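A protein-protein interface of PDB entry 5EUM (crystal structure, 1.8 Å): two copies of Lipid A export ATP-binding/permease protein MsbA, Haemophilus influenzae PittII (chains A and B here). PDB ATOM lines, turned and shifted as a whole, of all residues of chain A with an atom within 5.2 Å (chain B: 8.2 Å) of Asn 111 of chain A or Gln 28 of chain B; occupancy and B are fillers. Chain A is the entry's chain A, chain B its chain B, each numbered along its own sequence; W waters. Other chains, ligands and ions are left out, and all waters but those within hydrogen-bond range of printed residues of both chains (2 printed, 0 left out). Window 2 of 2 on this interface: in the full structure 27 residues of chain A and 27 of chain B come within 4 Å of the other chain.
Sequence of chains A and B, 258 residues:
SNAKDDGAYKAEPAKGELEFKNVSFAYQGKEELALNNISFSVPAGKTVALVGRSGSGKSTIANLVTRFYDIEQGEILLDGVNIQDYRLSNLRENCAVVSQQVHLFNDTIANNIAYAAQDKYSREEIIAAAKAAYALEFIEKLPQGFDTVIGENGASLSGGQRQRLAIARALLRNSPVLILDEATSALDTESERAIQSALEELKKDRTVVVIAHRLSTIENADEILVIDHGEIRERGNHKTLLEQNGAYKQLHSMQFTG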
ATOM      1  N   PHE A 105      -4.520  12.102 -17.215  1.00  0.00           N
ATOM      2  CA  PHE A 105      -3.301  11.433 -17.618  1.00  0.00           C
ATOM      3  C   PHE A 105      -2.261  12.424 -18.074  1.00  0.00           C
ATOM      4  O   PHE A 105      -2.593  13.551 -18.467  1.00  0.00           O
ATOM      5  CB  PHE A 105      -3.642  10.502 -18.787  1.00  0.00           C
ATOM      6  CG  PHE A 105      -4.499  11.161 -19.847  1.00  0.00           C
ATOM      7  CD1 PHE A 105      -5.898  11.160 -19.741  1.00  0.00           C
ATOM      8  CD2 PHE A 105      -3.923  11.806 -20.926  1.00  0.00           C
ATOM      9  CE1 PHE A 105      -6.686  11.775 -20.713  1.00  0.00           C
ATOM     10  CE2 PHE A 105      -4.709  12.413 -21.902  1.00  0.00           C
ATOM     11  CZ  PHE A 105      -6.084  12.400 -21.797  1.00  0.00           C
ATOM     12  N   ASP A 107      -0.408  14.597 -20.175  1.00  0.00           N
ATOM     13  CA  ASP A 107      -0.673  15.174 -21.494  1.00  0.00           C
ATOM     14  C   ASP A 107      -1.021  16.646 -21.199  1.00  0.00           C
ATOM     15  O   ASP A 107      -1.069  17.065 -20.034  1.00  0.00           O
ATOM     16  CB  ASP A 107      -1.867  14.501 -22.183  1.00  0.00           C
ATOM     17  CG  ASP A 107      -1.832  14.610 -23.697  1.00  0.00           C
ATOM     18  OD1 ASP A 107      -1.380  15.639 -24.252  1.00  0.00           O
ATOM     19  OD2 ASP A 107      -2.272  13.648 -24.347  1.00  0.00           O
ATOM     20  N   THR A 108      -1.283  17.421 -22.230  1.00  0.00           N
ATOM     21  CA  THR A 108      -1.654  18.817 -22.018  1.00  0.00           C
ATOM     22  C   THR A 108      -3.048  18.933 -21.427  1.00  0.00           C
ATOM     23  O   THR A 108      -3.853  18.009 -21.523  1.00  0.00           O
ATOM     24  CB  THR A 108      -1.611  19.615 -23.345  1.00  0.00           C
ATOM     25  OG1 THR A 108      -2.637  19.172 -24.245  1.00  0.00           O
ATOM     26  CG2 THR A 108      -0.264  19.467 -24.008  1.00  0.00           C
ATOM     27  N   ILE A 109      -3.322  20.072 -20.795  1.00  0.00           N
ATOM     28  CA  ILE A 109      -4.649  20.349 -20.250  1.00  0.00           C
ATOM     29  C   ILE A 109      -5.687  20.257 -21.388  1.00  0.00           C
ATOM     30  O   ILE A 109      -6.710  19.598 -21.238  1.00  0.00           O
ATOM     31  CB  ILE A 109      -4.669  21.721 -19.527  1.00  0.00           C
ATOM     32  CG1 ILE A 109      -3.772  21.651 -18.266  1.00  0.00           C
ATOM     33  CG2 ILE A 109      -6.095  22.144 -19.186  1.00  0.00           C
ATOM     34  CD1 ILE A 109      -3.674  22.943 -17.463  1.00  0.00           C
ATOM     35  N   ALA A 110      -5.394  20.877 -22.533  1.00  0.00           N
ATOM     36  CA  ALA A 110      -6.293  20.827 -23.692  1.00  0.00           C
ATOM     37  C   ALA A 110      -6.614  19.394 -24.120  1.00  0.00           C
ATOM     38  O   ALA A 110      -7.775  19.069 -24.347  1.00  0.00           O
ATOM     39  CB  ALA A 110      -5.707  21.590 -24.873  1.00  0.00           C
ATOM     40  N   ASN A 111      -5.595  18.541 -24.232  1.00  0.00           N
ATOM     41  CA  ASN A 111      -5.836  17.142 -24.638  1.00  0.00           C
ATOM     42  C   ASN A 111      -6.625  16.367 -23.590  1.00  0.00           C
ATOM     43  O   ASN A 111      -7.389  15.455 -23.929  1.00  0.00           O
ATOM     44  CB  ASN A 111      -4.538  16.425 -25.007  1.00  0.00           C
ATOM     45  CG  ASN A 111      -3.937  16.940 -26.309  1.00  0.00           C
ATOM     46  OD1 ASN A 111      -4.636  17.541 -27.150  1.00  0.00           O
ATOM     47  ND2 ASN A 111      -2.657  16.699 -26.498  1.00  0.00           N
ATOM     48  N   ASN A 112      -6.427  16.710 -22.320  1.00  0.00           N
ATOM     49  CA  ASN A 112      -7.222  16.089 -21.248  1.00  0.00           C
ATOM     50  C   ASN A 112      -8.677  16.503 -21.330  1.00  0.00           C
ATOM     51  O   ASN A 112      -9.562  15.721 -20.987  1.00  0.00           O
ATOM     52  CB  ASN A 112      -6.682  16.389 -19.846  1.00  0.00           C
ATOM     53  CG  ASN A 112      -5.642  15.376 -19.397  1.00  0.00           C
ATOM     54  OD1 ASN A 112      -5.986  14.376 -18.759  1.00  0.00           O
ATOM     55  ND2 ASN A 112      -4.383  15.590 -19.775  1.00  0.00           N
ATOM     56  N   ILE A 113      -8.928  17.749 -21.734  1.00  0.00           N
ATOM     57  CA  ILE A 113     -10.315  18.208 -21.884  1.00  0.00           C
ATOM     58  C   ILE A 113     -10.916  17.524 -23.115  1.00  0.00           C
ATOM     59  O   ILE A 113     -12.029  17.011 -23.052  1.00  0.00           O
ATOM     60  CB  ILE A 113     -10.416  19.741 -21.988  1.00  0.00           C
ATOM     61  CG1 ILE A 113      -9.994  20.387 -20.660  1.00  0.00           C
ATOM     62  CG2 ILE A 113     -11.844  20.156 -22.308  1.00  0.00           C
ATOM     63  CD1 ILE A 113      -9.894  21.902 -20.694  1.00  0.00           C
ATOM     64  N   ALA A 114     -10.167  17.498 -24.218  1.00  0.00           N
ATOM     65  CA  ALA A 114     -10.628  16.888 -25.476  1.00  0.00           C
ATOM     66  C   ALA A 114     -10.739  15.349 -25.493  1.00  0.00           C
ATOM     67  O   ALA A 114     -11.435  14.801 -26.348  1.00  0.00           O
ATOM     68  CB  ALA A 114      -9.774  17.363 -26.646  1.00  0.00           C
ATOM     69  N   TYR A 115     -10.075  14.656 -24.569  1.00  0.00           N
ATOM     70  CA  TYR A 115     -10.186  13.189 -24.463  1.00  0.00           C
ATOM     71  C   TYR A 115     -11.644  12.730 -24.688  1.00  0.00           C
ATOM     72  O   TYR A 115     -11.898  11.670 -25.256  1.00  0.00           O
ATOM     73  CB  TYR A 115      -9.702  12.787 -23.070  1.00  0.00           C
ATOM     74  CG  TYR A 115      -9.706  11.313 -22.732  1.00  0.00           C
ATOM     75  CD1 TYR A 115      -8.755  10.450 -23.277  1.00  0.00           C
ATOM     76  CD2 TYR A 115     -10.607  10.794 -21.794  1.00  0.00           C
ATOM     77  CE1 TYR A 115      -8.736   9.105 -22.945  1.00  0.00           C
ATOM     78  CE2 TYR A 115     -10.592   9.449 -21.452  1.00  0.00           C
ATOM     79  CZ  TYR A 115      -9.657   8.611 -22.031  1.00  0.00           C
ATOM     80  OH  TYR A 115      -9.634   7.278 -21.701  1.00  0.00           O
ATOM     81  N   LYS A 120     -13.383  15.537 -33.483  1.00  0.00           N
ATOM     82  CA  LYS A 120     -12.349  16.468 -33.019  1.00  0.00           C
ATOM     83  C   LYS A 120     -12.895  17.879 -32.791  1.00  0.00           C
ATOM     84  O   LYS A 120     -13.808  18.323 -33.483  1.00  0.00           O
ATOM     85  CB  LYS A 120     -11.173  16.518 -34.006  1.00  0.00           C
ATOM     86  CG  LYS A 120      -9.989  17.322 -33.482  1.00  0.00           C
ATOM     87  CD  LYS A 120      -8.826  17.389 -34.448  1.00  0.00           C
ATOM     88  CE  LYS A 120      -7.727  18.269 -33.872  1.00  0.00           C
ATOM     89  NZ  LYS A 120      -6.594  18.461 -34.823  1.00  0.00           N
ATOM     90  N   PHE B  25       8.560  10.391 -27.873  1.00  0.00           N
ATOM     91  CA  PHE B  25       7.123  10.654 -27.854  1.00  0.00           C
ATOM     92  C   PHE B  25       6.848  12.117 -27.547  1.00  0.00           C
ATOM     93  O   PHE B  25       7.487  12.714 -26.679  1.00  0.00           O
ATOM     94  CB  PHE B  25       6.465   9.758 -26.786  1.00  0.00           C
ATOM     95  CG  PHE B  25       4.972   9.942 -26.659  1.00  0.00           C
ATOM     96  CD1 PHE B  25       4.108   9.362 -27.574  1.00  0.00           C
ATOM     97  CD2 PHE B  25       4.440  10.673 -25.612  1.00  0.00           C
ATOM     98  CE1 PHE B  25       2.735   9.544 -27.478  1.00  0.00           C
ATOM     99  CE2 PHE B  25       3.069  10.851 -25.504  1.00  0.00           C
ATOM    100  CZ  PHE B  25       2.215  10.269 -26.428  1.00  0.00           C
ATOM    101  N   ALA B  26       5.871  12.680 -28.271  1.00  0.00           N
ATOM    102  CA  ALA B  26       5.413  14.036 -28.050  1.00  0.00           C
ATOM    103  C   ALA B  26       3.886  13.988 -27.973  1.00  0.00           C
ATOM    104  O   ALA B  26       3.229  13.229 -28.707  1.00  0.00           O
ATOM    105  CB  ALA B  26       5.858  14.956 -29.174  1.00  0.00           C
ATOM    106  N   TYR B  27       3.326  14.783 -27.071  1.00  0.00           N
ATOM    107  CA  TYR B  27       1.871  14.868 -26.933  1.00  0.00           C
ATOM    108  C   TYR B  27       1.318  15.518 -28.195  1.00  0.00           C
ATOM    109  O   TYR B  27       2.012  16.309 -28.837  1.00  0.00           O
ATOM    110  CB  TYR B  27       1.490  15.694 -25.704  1.00  0.00           C
ATOM    111  CG  TYR B  27       2.047  15.103 -24.425  1.00  0.00           C
ATOM    112  CD1 TYR B  27       1.666  13.847 -24.025  1.00  0.00           C
ATOM    113  CD2 TYR B  27       2.950  15.805 -23.624  1.00  0.00           C
ATOM    114  CE1 TYR B  27       2.187  13.269 -22.874  1.00  0.00           C
ATOM    115  CE2 TYR B  27       3.460  15.239 -22.449  1.00  0.00           C
ATOM    116  CZ  TYR B  27       3.078  13.962 -22.090  1.00  0.00           C
ATOM    117  OH  TYR B  27       3.555  13.342 -20.934  1.00  0.00           O
ATOM    118  N   GLN B  28       0.090  15.157 -28.556  1.00  0.00           N
ATOM    119  CA  GLN B  28      -0.567  15.710 -29.744  1.00  0.00           C
ATOM    120  C   GLN B  28      -0.598  17.230 -29.649  1.00  0.00           C
ATOM    121  O   GLN B  28      -1.001  17.777 -28.624  1.00  0.00           O
ATOM    122  CB  GLN B  28      -1.977  15.138 -29.849  1.00  0.00           C
ATOM    123  CG  GLN B  28      -2.867  15.755 -30.909  1.00  0.00           C
ATOM    124  CD  GLN B  28      -4.237  15.102 -30.913  1.00  0.00           C
ATOM    125  OE1 GLN B  28      -4.363  13.909 -31.197  1.00  0.00           O
ATOM    126  NE2 GLN B  28      -5.273  15.879 -30.600  1.00  0.00           N
ATOM    127  N   GLY B  29      -0.166  17.910 -30.708  1.00  0.00           N
ATOM    128  CA  GLY B  29      -0.136  19.376 -30.723  1.00  0.00           C
ATOM    129  C   GLY B  29       1.089  20.020 -30.075  1.00  0.00           C
ATOM    130  O   GLY B  29       1.110  21.242 -29.892  1.00  0.00           O
ATOM    131  N   MLZ B  30       2.096  19.215 -29.703  1.00  0.00           N
ATOM    132  CA  MLZ B  30       3.343  19.730 -29.104  1.00  0.00           C
ATOM    133  CB  MLZ B  30       3.656  19.135 -27.713  1.00  0.00           C
ATOM    134  CG  MLZ B  30       2.845  19.750 -26.569  1.00  0.00           C
ATOM    135  CD  MLZ B  30       3.739  20.401 -25.519  1.00  0.00           C
ATOM    136  CE  MLZ B  30       2.950  21.192 -24.489  1.00  0.00           C
ATOM    137  NZ  MLZ B  30       3.635  22.395 -24.013  1.00  0.00           N
ATOM    138  CM  MLZ B  30       4.432  22.420 -22.794  1.00  0.00           C
ATOM    139  C   MLZ B  30       4.496  19.324 -29.988  1.00  0.00           C
ATOM    140  O   MLZ B  30       4.557  18.175 -30.459  1.00  0.00           O
ATOM    141  N   GLU B  31       5.420  20.254 -30.226  1.00  0.00           N
ATOM    142  CA  GLU B  31       6.624  19.962 -31.007  1.00  0.00           C
ATOM    143  C   GLU B  31       7.714  19.376 -30.085  1.00  0.00           C
ATOM    144  O   GLU B  31       8.458  18.478 -30.485  1.00  0.00           O
ATOM    145  CB  GLU B  31       7.143  21.222 -31.724  1.00  0.00           C
ATOM    146  CG  GLU B  31       8.389  20.968 -32.578  1.00  0.00           C
ATOM    147  CD  GLU B  31       8.878  22.193 -33.343  1.00  0.00           C
ATOM    148  OE1 GLU B  31       8.094  23.147 -33.541  1.00  0.00           O
ATOM    149  OE2 GLU B  31      10.058  22.186 -33.760  1.00  0.00           O
ATOM    150  N   GLU B  32       7.792  19.883 -28.857  1.00  0.00           N
ATOM    151  CA  GLU B  32       8.789  19.431 -27.879  1.00  0.00           C
ATOM    152  C   GLU B  32       8.512  17.986 -27.457  1.00  0.00           C
ATOM    153  O   GLU B  32       7.361  17.572 -27.357  1.00  0.00           O
ATOM    154  CB  GLU B  32       8.757  20.353 -26.657  1.00  0.00           C
ATOM    155  CG  GLU B  32       9.844  20.109 -25.625  1.00  0.00           C
ATOM    156  CD  GLU B  32       9.783  21.087 -24.461  1.00  0.00           C
ATOM    157  OE1 GLU B  32       8.767  21.813 -24.335  1.00  0.00           O
ATOM    158  OE2 GLU B  32      10.752  21.123 -23.667  1.00  0.00           O
ATOM    159  N   PHE B  68      -1.859   3.462 -23.814  1.00  0.00           N
ATOM    160  CA  PHE B  68      -2.797   4.545 -23.518  1.00  0.00           C
ATOM    161  C   PHE B  68      -2.724   5.534 -24.708  1.00  0.00           C
ATOM    162  O   PHE B  68      -3.720   6.152 -25.107  1.00  0.00           O
ATOM    163  CB  PHE B  68      -2.505   5.234 -22.197  1.00  0.00           C
ATOM    164  CG  PHE B  68      -3.471   6.323 -21.902  1.00  0.00           C
ATOM    165  CD1 PHE B  68      -4.741   6.023 -21.422  1.00  0.00           C
ATOM    166  CD2 PHE B  68      -3.140   7.644 -22.156  1.00  0.00           C
ATOM    167  CE1 PHE B  68      -5.653   7.029 -21.178  1.00  0.00           C
ATOM    168  CE2 PHE B  68      -4.049   8.653 -21.912  1.00  0.00           C
ATOM    169  CZ  PHE B  68      -5.307   8.345 -21.421  1.00  0.00           C
ATOM    170  N   TYR B  69      -1.522   5.632 -25.255  1.00  0.00           N
ATOM    171  CA  TYR B  69      -1.200   6.351 -26.485  1.00  0.00           C
ATOM    172  C   TYR B  69      -0.119   5.524 -27.206  1.00  0.00           C
ATOM    173  O   TYR B  69       0.535   4.665 -26.589  1.00  0.00           O
ATOM    174  CB  TYR B  69      -0.830   7.854 -26.312  1.00  0.00           C
ATOM    175  CG  TYR B  69      -0.432   8.369 -24.931  1.00  0.00           C
ATOM    176  CD1 TYR B  69       0.556   7.766 -24.180  1.00  0.00           C
ATOM    177  CD2 TYR B  69      -1.016   9.534 -24.420  1.00  0.00           C
ATOM    178  CE1 TYR B  69       0.926   8.256 -22.928  1.00  0.00           C
ATOM    179  CE2 TYR B  69      -0.656  10.038 -23.183  1.00  0.00           C
ATOM    180  CZ  TYR B  69       0.306   9.398 -22.427  1.00  0.00           C
ATOM    181  OH  TYR B  69       0.663   9.908 -21.178  1.00  0.00           O
HETATM  182  O   HOH W   1      -1.336  13.513 -26.948  1.00  0.00           O
HETATM  183  O   HOH W   2      -2.480  20.094 -26.694  1.00  0.00           O
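The side-chain amide nitrogen of Asn 111 of chain A lies within hydrogen-bond range of the backbone carbonyl oxygen of Gln 28 of chain B (2.9 Å).
O of Phe 105 of chain A lies within hydrogen-bond range of ND2 of Asn 112 of chain A (3.0 Å). OD1 of Asp 107 of chain A is in hydrogen-bond range of ND2 of Asn 111 of chain A (2.8 Å). The side-chain hydroxyl (OG1) of Thr 108 of chain A is in hydrogen-bond range of the backbone NH (N) of Asn 111 of chain A (3.0 Å). O of Thr 108 of chain A is in hydrogen-bond range of ND2 of Asn 112 of chain A (3.0 Å).
Among the printed residues, pairs that only touch across the chains: Asp 107 of chain A with Tyr 27 of chain B (3.2 Å), Phe 105 of chain A with Phe 68 of chain B (3.3 Å), Thr 108 of chain A with MLZ 30 of chain B (3.7 Å) and Tyr 115 of chain A with Phe 68 of chain B (3.8 Å).
Printed residues of chain B within 4 Å of Asn 111 of chain A: Gln 28. Of chain A, only Asn 111 comes within 4 Å of Gln 28 of chain B. Ala 110 of chain A touches none of the printed residues of chain B. Of the printed residues of chain B, Tyr 115 of chain A touches Phe 68 (3.8 Å). Of the printed residues of chain A, Phe 68 of chain B touches Phe 105 (3.3 Å) and Tyr 115 (3.8 Å). Printed residues of chain B within 4 Å of Asp 107 of chain A: Tyr 27. Phe 25 of chain B touches none of the printed residues of chain A. Ile 113 of chain A touches none of the printed residues of chain B. The nearest residue of chain B that does not touch Asn 111 of chain A is Tyr 27 of chain B (4.3 Å).
Of the 11 printed residues of chain A, 5 touch a printed residue of chain B. Printed residues of chain A that touch a printed residue of chain B: Phe 105, Asp 107, Thr 108, Asn 111 and Tyr 115. Of the 10 printed residues of chain B, 4 touch a printed residue of chain A. Hydrophobic or aromatic side chains of chain B within 4 Å of the printed part of chain A: Tyr 27 and Phe 68. Among the printed residues, 5 pairs touch across the chains.
No position is printed for both chains. Of the 5 pairs that touch across the chains among the printed residues, none has its exchanged pair printed and touching as well.
Water W2 lies within hydrogen-bond range of the side-chain hydroxyl of Thr 108 of chain A (2.6 Å), the backbone carbonyl oxygen of Gln 28 of chain B (3.4 Å) and the side-chain amide oxygen of Asn 111 of chain A (3.4 Å). Water W1 lies within hydrogen-bond range of the backbone NH (N) of Gln 28 of chain B (2.7 Å), the side-chain carboxylate (OD2) of Asp 107 of chain A (2.8 Å) and the side-chain amide nitrogen (ND2) of Asn 111 of chain A (3.5 Å).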
